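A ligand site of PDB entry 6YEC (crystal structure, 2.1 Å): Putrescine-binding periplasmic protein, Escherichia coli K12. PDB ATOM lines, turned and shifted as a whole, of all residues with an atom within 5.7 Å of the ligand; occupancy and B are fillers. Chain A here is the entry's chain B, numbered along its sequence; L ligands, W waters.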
ATOM      1  N   TRP A  11      12.150  17.388  -1.281  1.00  0.00           N
ATOM      2  CA  TRP A  11      13.590  17.181  -1.115  1.00  0.00           C
ATOM      3  C   TRP A  11      13.918  16.884   0.347  1.00  0.00           C
ATOM      4  O   TRP A  11      13.160  17.200   1.261  1.00  0.00           O
ATOM      5  CB  TRP A  11      14.365  18.405  -1.575  1.00  0.00           C
ATOM      6  CG  TRP A  11      14.163  18.784  -3.011  1.00  0.00           C
ATOM      7  CD1 TRP A  11      13.095  19.470  -3.528  1.00  0.00           C
ATOM      8  CD2 TRP A  11      15.040  18.515  -4.106  1.00  0.00           C
ATOM      9  NE1 TRP A  11      13.264  19.639  -4.879  1.00  0.00           N
ATOM     10  CE2 TRP A  11      14.441  19.067  -5.261  1.00  0.00           C
ATOM     11  CE3 TRP A  11      16.269  17.863  -4.225  1.00  0.00           C
ATOM     12  CZ2 TRP A  11      15.033  18.975  -6.521  1.00  0.00           C
ATOM     13  CZ3 TRP A  11      16.852  17.778  -5.477  1.00  0.00           C
ATOM     14  CH2 TRP A  11      16.239  18.333  -6.614  1.00  0.00           C
ATOM     15  N   SER A  12      15.076  16.262   0.559  1.00  0.00           N
ATOM     16  CA  SER A  12      15.554  16.028   1.912  1.00  0.00           C
ATOM     17  C   SER A  12      15.963  17.340   2.567  1.00  0.00           C
ATOM     18  O   SER A  12      16.449  18.252   1.897  1.00  0.00           O
ATOM     19  CB  SER A  12      16.737  15.056   1.904  1.00  0.00           C
ATOM     20  OG  SER A  12      17.652  15.387   0.875  1.00  0.00           O
ATOM     21  N   ASP A  13      15.761  17.424   3.878  1.00  0.00           N
ATOM     22  CA  ASP A  13      16.116  18.601   4.662  1.00  0.00           C
ATOM     23  C   ASP A  13      15.589  19.884   4.017  1.00  0.00           C
ATOM     24  O   ASP A  13      16.283  20.891   3.899  1.00  0.00           O
ATOM     25  CB  ASP A  13      17.632  18.680   4.873  1.00  0.00           C
ATOM     26  CG  ASP A  13      18.202  17.424   5.496  1.00  0.00           C
ATOM     27  OD1 ASP A  13      17.600  16.915   6.471  1.00  0.00           O
ATOM     28  OD2 ASP A  13      19.255  16.951   5.031  1.00  0.00           O
ATOM     29  N   TYR A  14      14.320  19.840   3.600  1.00  0.00           N
ATOM     30  CA  TYR A  14      13.697  20.945   2.872  1.00  0.00           C
ATOM     31  C   TYR A  14      12.434  21.418   3.573  1.00  0.00           C
ATOM     32  O   TYR A  14      11.534  21.974   2.934  1.00  0.00           O
ATOM     33  CB  TYR A  14      13.399  20.537   1.434  1.00  0.00           C
ATOM     34  CG  TYR A  14      13.739  21.605   0.419  1.00  0.00           C
ATOM     35  CD1 TYR A  14      14.698  22.574   0.695  1.00  0.00           C
ATOM     36  CD2 TYR A  14      13.114  21.639  -0.825  1.00  0.00           C
ATOM     37  CE1 TYR A  14      15.014  23.544  -0.233  1.00  0.00           C
ATOM     38  CE2 TYR A  14      13.430  22.609  -1.753  1.00  0.00           C
ATOM     39  CZ  TYR A  14      14.374  23.559  -1.456  1.00  0.00           C
ATOM     40  OH  TYR A  14      14.693  24.519  -2.386  1.00  0.00           O
ATOM     41  N   ASP A  37      16.210  13.035  -3.403  1.00  0.00           N
ATOM     42  CA  ASP A  37      17.443  13.809  -3.461  1.00  0.00           C
ATOM     43  C   ASP A  37      17.877  14.139  -4.885  1.00  0.00           C
ATOM     44  O   ASP A  37      19.031  14.530  -5.097  1.00  0.00           O
ATOM     45  CB  ASP A  37      18.577  13.078  -2.737  1.00  0.00           C
ATOM     46  CG  ASP A  37      18.231  12.729  -1.306  1.00  0.00           C
ATOM     47  OD1 ASP A  37      17.429  11.788  -1.084  1.00  0.00           O
ATOM     48  OD2 ASP A  37      18.752  13.396  -0.388  1.00  0.00           O
ATOM     49  N   ASN A  39      16.347  15.557  -9.014  1.00  0.00           N
ATOM     50  CA  ASN A  39      15.282  15.886  -9.959  1.00  0.00           C
ATOM     51  C   ASN A  39      14.982  14.711 -10.887  1.00  0.00           C
ATOM     52  O   ASN A  39      13.834  14.492 -11.268  1.00  0.00           O
ATOM     53  CB  ASN A  39      15.656  17.123 -10.770  1.00  0.00           C
ATOM     54  CG  ASN A  39      15.141  18.406 -10.132  1.00  0.00           C
ATOM     55  OD1 ASN A  39      13.964  18.527  -9.818  1.00  0.00           O
ATOM     56  ND2 ASN A  39      16.036  19.366  -9.950  1.00  0.00           N
ATOM     57  N   SER A  59      12.042  21.129  -9.419  1.00  0.00           N
ATOM     58  CA  SER A  59      12.601  22.392  -9.845  1.00  0.00           C
ATOM     59  C   SER A  59      11.782  22.966 -10.989  1.00  0.00           C
ATOM     60  O   SER A  59      11.171  22.237 -11.776  1.00  0.00           O
ATOM     61  CB  SER A  59      14.063  22.226 -10.275  1.00  0.00           C
ATOM     62  OG  SER A  59      14.880  21.930  -9.149  1.00  0.00           O
ATOM     63  N   SER A  61      12.674  24.434 -13.721  1.00  0.00           N
ATOM     64  CA  SER A  61      13.166  24.084 -15.048  1.00  0.00           C
ATOM     65  C   SER A  61      12.743  22.687 -15.455  1.00  0.00           C
ATOM     66  O   SER A  61      12.504  22.424 -16.638  1.00  0.00           O
ATOM     67  CB  SER A  61      14.688  24.218 -15.104  1.00  0.00           C
ATOM     68  OG  SER A  61      15.312  23.270 -14.256  1.00  0.00           O
ATOM     69  N   PHE A  62      12.639  21.758 -14.490  1.00  0.00           N
ATOM     70  CA  PHE A  62      12.147  20.418 -14.807  1.00  0.00           C
ATOM     71  C   PHE A  62      10.637  20.373 -14.919  1.00  0.00           C
ATOM     72  O   PHE A  62      10.101  19.567 -15.691  1.00  0.00           O
ATOM     73  CB  PHE A  62      12.631  19.422 -13.755  1.00  0.00           C
ATOM     74  CG  PHE A  62      14.045  18.974 -13.951  1.00  0.00           C
ATOM     75  CD1 PHE A  62      15.108  19.786 -13.591  1.00  0.00           C
ATOM     76  CD2 PHE A  62      14.312  17.731 -14.500  1.00  0.00           C
ATOM     77  CE1 PHE A  62      16.418  19.370 -13.776  1.00  0.00           C
ATOM     78  CE2 PHE A  62      15.617  17.305 -14.693  1.00  0.00           C
ATOM     79  CZ  PHE A  62      16.671  18.123 -14.324  1.00  0.00           C
ATOM     80  N   GLU A 158      23.504  19.850 -16.628  1.00  0.00           N
ATOM     81  CA  GLU A 158      22.872  21.087 -17.080  1.00  0.00           C
ATOM     82  C   GLU A 158      23.373  22.295 -16.302  1.00  0.00           C
ATOM     83  O   GLU A 158      23.553  23.375 -16.862  1.00  0.00           O
ATOM     84  CB  GLU A 158      21.342  20.964 -16.985  1.00  0.00           C
ATOM     85  CG  GLU A 158      20.794  20.744 -15.579  1.00  0.00           C
ATOM     86  CD  GLU A 158      21.009  19.336 -15.059  1.00  0.00           C
ATOM     87  OE1 GLU A 158      20.922  19.131 -13.832  1.00  0.00           O
ATOM     88  OE2 GLU A 158      21.273  18.433 -15.884  1.00  0.00           O
ATOM     89  N   GLU A 159      23.622  22.124 -14.997  1.00  0.00           N
ATOM     90  CA  GLU A 159      24.089  23.230 -14.180  1.00  0.00           C
ATOM     91  C   GLU A 159      25.578  23.490 -14.384  1.00  0.00           C
ATOM     92  O   GLU A 159      26.012  24.646 -14.444  1.00  0.00           O
ATOM     93  CB  GLU A 159      23.793  22.971 -12.712  1.00  0.00           C
ATOM     94  CG  GLU A 159      22.335  22.658 -12.412  1.00  0.00           C
ATOM     95  CD  GLU A 159      22.061  22.477 -10.933  1.00  0.00           C
ATOM     96  OE1 GLU A 159      22.825  23.042 -10.121  1.00  0.00           O
ATOM     97  OE2 GLU A 159      21.098  21.772 -10.580  1.00  0.00           O
ATOM     98  N   ILE A 204      27.873  17.716   1.121  1.00  0.00           N
ATOM     99  CA  ILE A 204      27.386  18.399   2.321  1.00  0.00           C
ATOM    100  C   ILE A 204      28.134  17.914   3.555  1.00  0.00           C
ATOM    101  O   ILE A 204      28.789  18.695   4.250  1.00  0.00           O
ATOM    102  CB  ILE A 204      25.869  18.194   2.473  1.00  0.00           C
ATOM    103  CG1 ILE A 204      25.135  18.704   1.235  1.00  0.00           C
ATOM    104  CG2 ILE A 204      25.360  18.891   3.729  1.00  0.00           C
ATOM    105  CD1 ILE A 204      23.656  18.433   1.241  1.00  0.00           C
ATOM    106  N   TRP A 218      24.741  23.714  -4.079  1.00  0.00           N
ATOM    107  CA  TRP A 218      23.638  24.633  -3.910  1.00  0.00           C
ATOM    108  C   TRP A 218      23.754  25.360  -2.577  1.00  0.00           C
ATOM    109  O   TRP A 218      24.212  24.791  -1.580  1.00  0.00           O
ATOM    110  CB  TRP A 218      22.303  23.886  -4.015  1.00  0.00           C
ATOM    111  CG  TRP A 218      22.192  23.130  -5.302  1.00  0.00           C
ATOM    112  CD1 TRP A 218      22.391  23.627  -6.560  1.00  0.00           C
ATOM    113  CD2 TRP A 218      21.882  21.737  -5.471  1.00  0.00           C
ATOM    114  NE1 TRP A 218      22.211  22.645  -7.501  1.00  0.00           N
ATOM    115  CE2 TRP A 218      21.902  21.470  -6.854  1.00  0.00           C
ATOM    116  CE3 TRP A 218      21.597  20.701  -4.587  1.00  0.00           C
ATOM    117  CZ2 TRP A 218      21.639  20.203  -7.376  1.00  0.00           C
ATOM    118  CZ3 TRP A 218      21.331  19.443  -5.107  1.00  0.00           C
ATOM    119  CH2 TRP A 218      21.356  19.208  -6.486  1.00  0.00           C
ATOM    120  N   ASP A 221      22.352  24.015   0.796  1.00  0.00           N
ATOM    121  CA  ASP A 221      23.062  22.799   1.199  1.00  0.00           C
ATOM    122  C   ASP A 221      24.395  23.142   1.844  1.00  0.00           C
ATOM    123  O   ASP A 221      24.779  22.528   2.857  1.00  0.00           O
ATOM    124  CB  ASP A 221      23.267  21.893  -0.009  1.00  0.00           C
ATOM    125  CG  ASP A 221      21.969  21.375  -0.580  1.00  0.00           C
ATOM    126  OD1 ASP A 221      20.898  21.873  -0.159  1.00  0.00           O
ATOM    127  OD2 ASP A 221      22.006  20.481  -1.447  1.00  0.00           O
ATOM    128  N   GLN A 224      23.745  24.582   5.270  1.00  0.00           N
ATOM    129  CA  GLN A 224      23.408  23.502   6.190  1.00  0.00           C
ATOM    130  C   GLN A 224      24.663  22.730   6.603  1.00  0.00           C
ATOM    131  O   GLN A 224      24.801  22.344   7.772  1.00  0.00           O
ATOM    132  CB  GLN A 224      22.385  22.556   5.550  1.00  0.00           C
ATOM    133  CG  GLN A 224      20.974  23.128   5.506  1.00  0.00           C
ATOM    134  CD  GLN A 224      19.993  22.201   4.828  1.00  0.00           C
ATOM    135  OE1 GLN A 224      20.044  20.979   4.988  1.00  0.00           O
ATOM    136  NE2 GLN A 224      19.085  22.774   4.041  1.00  0.00           N
ATOM    137  N   ARG A 228      26.112  22.465  10.398  1.00  0.00           N
ATOM    138  CA  ARG A 228      26.462  21.213  11.065  1.00  0.00           C
ATOM    139  C   ARG A 228      27.883  21.252  11.612  1.00  0.00           C
ATOM    140  O   ARG A 228      28.161  20.626  12.644  1.00  0.00           O
ATOM    141  CB  ARG A 228      26.332  20.028  10.106  1.00  0.00           C
ATOM    142  CG  ARG A 228      24.924  19.691   9.644  1.00  0.00           C
ATOM    143  CD  ARG A 228      24.992  18.588   8.594  1.00  0.00           C
ATOM    144  NE  ARG A 228      23.715  18.373   7.912  1.00  0.00           N
ATOM    145  CZ  ARG A 228      23.524  17.413   7.013  1.00  0.00           C
ATOM    146  NH1 ARG A 228      24.514  16.588   6.686  1.00  0.00           N
ATOM    147  NH2 ARG A 228      22.337  17.276   6.433  1.00  0.00           N
ATOM    148  N   MET A 248      24.145  30.376 -11.651  1.00  0.00           N
ATOM    149  CA  MET A 248      22.825  29.870 -11.993  1.00  0.00           C
ATOM    150  C   MET A 248      21.912  29.937 -10.782  1.00  0.00           C
ATOM    151  O   MET A 248      22.306  29.599  -9.660  1.00  0.00           O
ATOM    152  CB  MET A 248      22.908  28.431 -12.501  1.00  0.00           C
ATOM    153  CG  MET A 248      21.617  27.926 -13.127  1.00  0.00           C
ATOM    154  SD  MET A 248      21.392  26.149 -12.894  1.00  0.00           S
ATOM    155  CE  MET A 248      20.931  26.098 -11.160  1.00  0.00           C
ATOM    156  N   PHE A 250      18.032  28.735  -9.266  1.00  0.00           N
ATOM    157  CA  PHE A 250      16.988  27.732  -9.436  1.00  0.00           C
ATOM    158  C   PHE A 250      15.836  28.039  -8.488  1.00  0.00           C
ATOM    159  O   PHE A 250      16.008  28.717  -7.466  1.00  0.00           O
ATOM    160  CB  PHE A 250      17.516  26.316  -9.181  1.00  0.00           C
ATOM    161  CG  PHE A 250      18.049  26.081  -7.799  1.00  0.00           C
ATOM    162  CD1 PHE A 250      17.228  25.621  -6.788  1.00  0.00           C
ATOM    163  CD2 PHE A 250      19.391  26.318  -7.512  1.00  0.00           C
ATOM    164  CE1 PHE A 250      17.717  25.406  -5.514  1.00  0.00           C
ATOM    165  CE2 PHE A 250      19.885  26.106  -6.245  1.00  0.00           C
ATOM    166  CZ  PHE A 250      19.057  25.646  -5.240  1.00  0.00           C
ATOM    167  N   ASP A 252      12.660  25.982  -6.639  1.00  0.00           N
ATOM    168  CA  ASP A 252      11.913  24.781  -6.308  1.00  0.00           C
ATOM    169  C   ASP A 252      10.469  25.150  -6.020  1.00  0.00           C
ATOM    170  O   ASP A 252      10.191  26.084  -5.261  1.00  0.00           O
ATOM    171  CB  ASP A 252      12.534  24.066  -5.097  1.00  0.00           C
ATOM    172  CG  ASP A 252      13.854  23.398  -5.433  1.00  0.00           C
ATOM    173  OD1 ASP A 252      14.020  22.946  -6.590  1.00  0.00           O
ATOM    174  OD2 ASP A 252      14.727  23.333  -4.543  1.00  0.00           O
ATOM    175  N   TYR A 288      17.359  28.254   3.315  1.00  0.00           N
ATOM    176  CA  TYR A 288      16.978  28.581   1.944  1.00  0.00           C
ATOM    177  C   TYR A 288      16.081  29.812   1.950  1.00  0.00           C
ATOM    178  O   TYR A 288      15.221  29.961   2.821  1.00  0.00           O
ATOM    179  CB  TYR A 288      16.238  27.413   1.275  1.00  0.00           C
ATOM    180  CG  TYR A 288      17.142  26.387   0.622  1.00  0.00           C
ATOM    181  CD1 TYR A 288      17.525  26.514  -0.698  1.00  0.00           C
ATOM    182  CD2 TYR A 288      17.595  25.281   1.336  1.00  0.00           C
ATOM    183  CE1 TYR A 288      18.342  25.571  -1.304  1.00  0.00           C
ATOM    184  CE2 TYR A 288      18.408  24.326   0.735  1.00  0.00           C
ATOM    185  CZ  TYR A 288      18.784  24.481  -0.580  1.00  0.00           C
ATOM    186  OH  TYR A 288      19.592  23.544  -1.176  1.00  0.00           O
ATOM    187  N   LEU A 322      18.228  28.531 -16.114  1.00  0.00           N
ATOM    188  CA  LEU A 322      18.325  27.508 -17.148  1.00  0.00           C
ATOM    189  C   LEU A 322      17.161  27.591 -18.112  1.00  0.00           C
ATOM    190  O   LEU A 322      16.007  27.807 -17.713  1.00  0.00           O
ATOM    191  CB  LEU A 322      18.381  26.119 -16.517  1.00  0.00           C
ATOM    192  CG  LEU A 322      19.753  25.613 -16.060  1.00  0.00           C
ATOM    193  CD1 LEU A 322      19.635  24.232 -15.442  1.00  0.00           C
ATOM    194  CD2 LEU A 322      20.726  25.606 -17.225  1.00  0.00           C
HETATM  195  N1  LIG L   1      19.791  17.690   1.647  1.00  0.00           N
HETATM  196  C1  LIG L   1      20.185  19.078   1.746  1.00  0.00           C
HETATM  197  C2  LIG L   1      18.991  19.921   1.329  1.00  0.00           C
HETATM  198  C3  LIG L   1      18.479  19.551  -0.061  1.00  0.00           C
HETATM  199  N2  LIG L   1      17.921  20.696  -0.747  1.00  0.00           N
HETATM  200  C4  LIG L   1      17.315  20.548  -2.052  1.00  0.00           C
HETATM  201  C5  LIG L   1      17.425  21.780  -2.940  1.00  0.00           C
HETATM  202  C6  LIG L   1      16.975  21.465  -4.364  1.00  0.00           C
HETATM  203  C7  LIG L   1      18.132  21.745  -5.332  1.00  0.00           C
HETATM  204  N3  LIG L   1      17.743  21.737  -6.728  1.00  0.00           N
HETATM  205  C8  LIG L   1      18.730  22.054  -7.748  1.00  0.00           C
HETATM  206  C9  LIG L   1      18.097  22.819  -8.906  1.00  0.00           C
HETATM  207  C10 LIG L   1      18.122  21.959 -10.171  1.00  0.00           C
HETATM  208  N4  LIG L   1      17.864  22.778 -11.346  1.00  0.00           N
HETATM  209  O   HOH W   1      16.880  24.972 -12.737  1.00  0.00           O
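Residues that only touch the ligand: Asn 39, Ser 59, Trp 218, Phe 250, Trp 11, Ile 204, Gln 224, Tyr 14 and Ser 61. Hydrophobic or aromatic side chains within 4 Å of the ligand: Trp 11, Tyr 14, Ile 204, Trp 218, Phe 250 and Tyr 288. Of the 21 residues printed, 15 come within 4 Å of the ligand. The nearest printed residue that does not touch the ligand is Phe 62 (4.4 Å).
Water W1 lies within hydrogen-bond range of the side-chain hydroxyl of Ser 61 and a nitrogen (N4) of the ligand.
The side-chain hydroxyl (OG) of Ser 59 lies within hydrogen-bond range of the side-chain carboxylate (OD1) of Asp 252. The side-chain carboxylate (OD2) of Asp 252 is in hydrogen-bond range of the side-chain hydroxyl (OH) of Tyr 14 (2.5 Å). The side-chain carboxylate (OE1) of Glu 159 sits at hydrogen-bond distance from the indole nitrogen (NE1) of Trp 218, at 2.7 Å. OG of Ser 12 lies within hydrogen-bond range of OD2 of Asp 37, at 2.6 Å. N of Asp 221 lies close to OH of Tyr 288 (3.4 Å). OG of Ser 59 is in hydrogen-bond range of ND2 of Asn 39 (2.9 Å). The side-chain amide nitrogen (NE2) of Gln 224 is in hydrogen-bond range of the backbone carbonyl oxygen (O) of Asp 13. The side-chain carboxylate of Asp 13 is in salt-bridge range of the guanidinium group of Arg 228 (3.4 Å).
N3 of the ligand lies within salt-bridge range of OD1 of Asp 252, 3.9 Å away. A nitrogen (N4) of the ligand is in salt-bridge range of the side-chain carboxylate of Glu 159 (3.5 Å). N1 of the ligand sits close to O of Ser 12, at 3.4 Å. OG of Ser 12 is in hydrogen-bond range of N1 of the ligand, at 3.2 Å. The side-chain carboxylate of Asp 221 is in salt-bridge range of a nitrogen (N2) of the ligand, at 3.3 Å. N2 of the ligand sits close to OH of Tyr 288 (3.3 Å). OD2 of Asp 13 lies within salt-bridge range of N1 of the ligand (3.5 Å).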
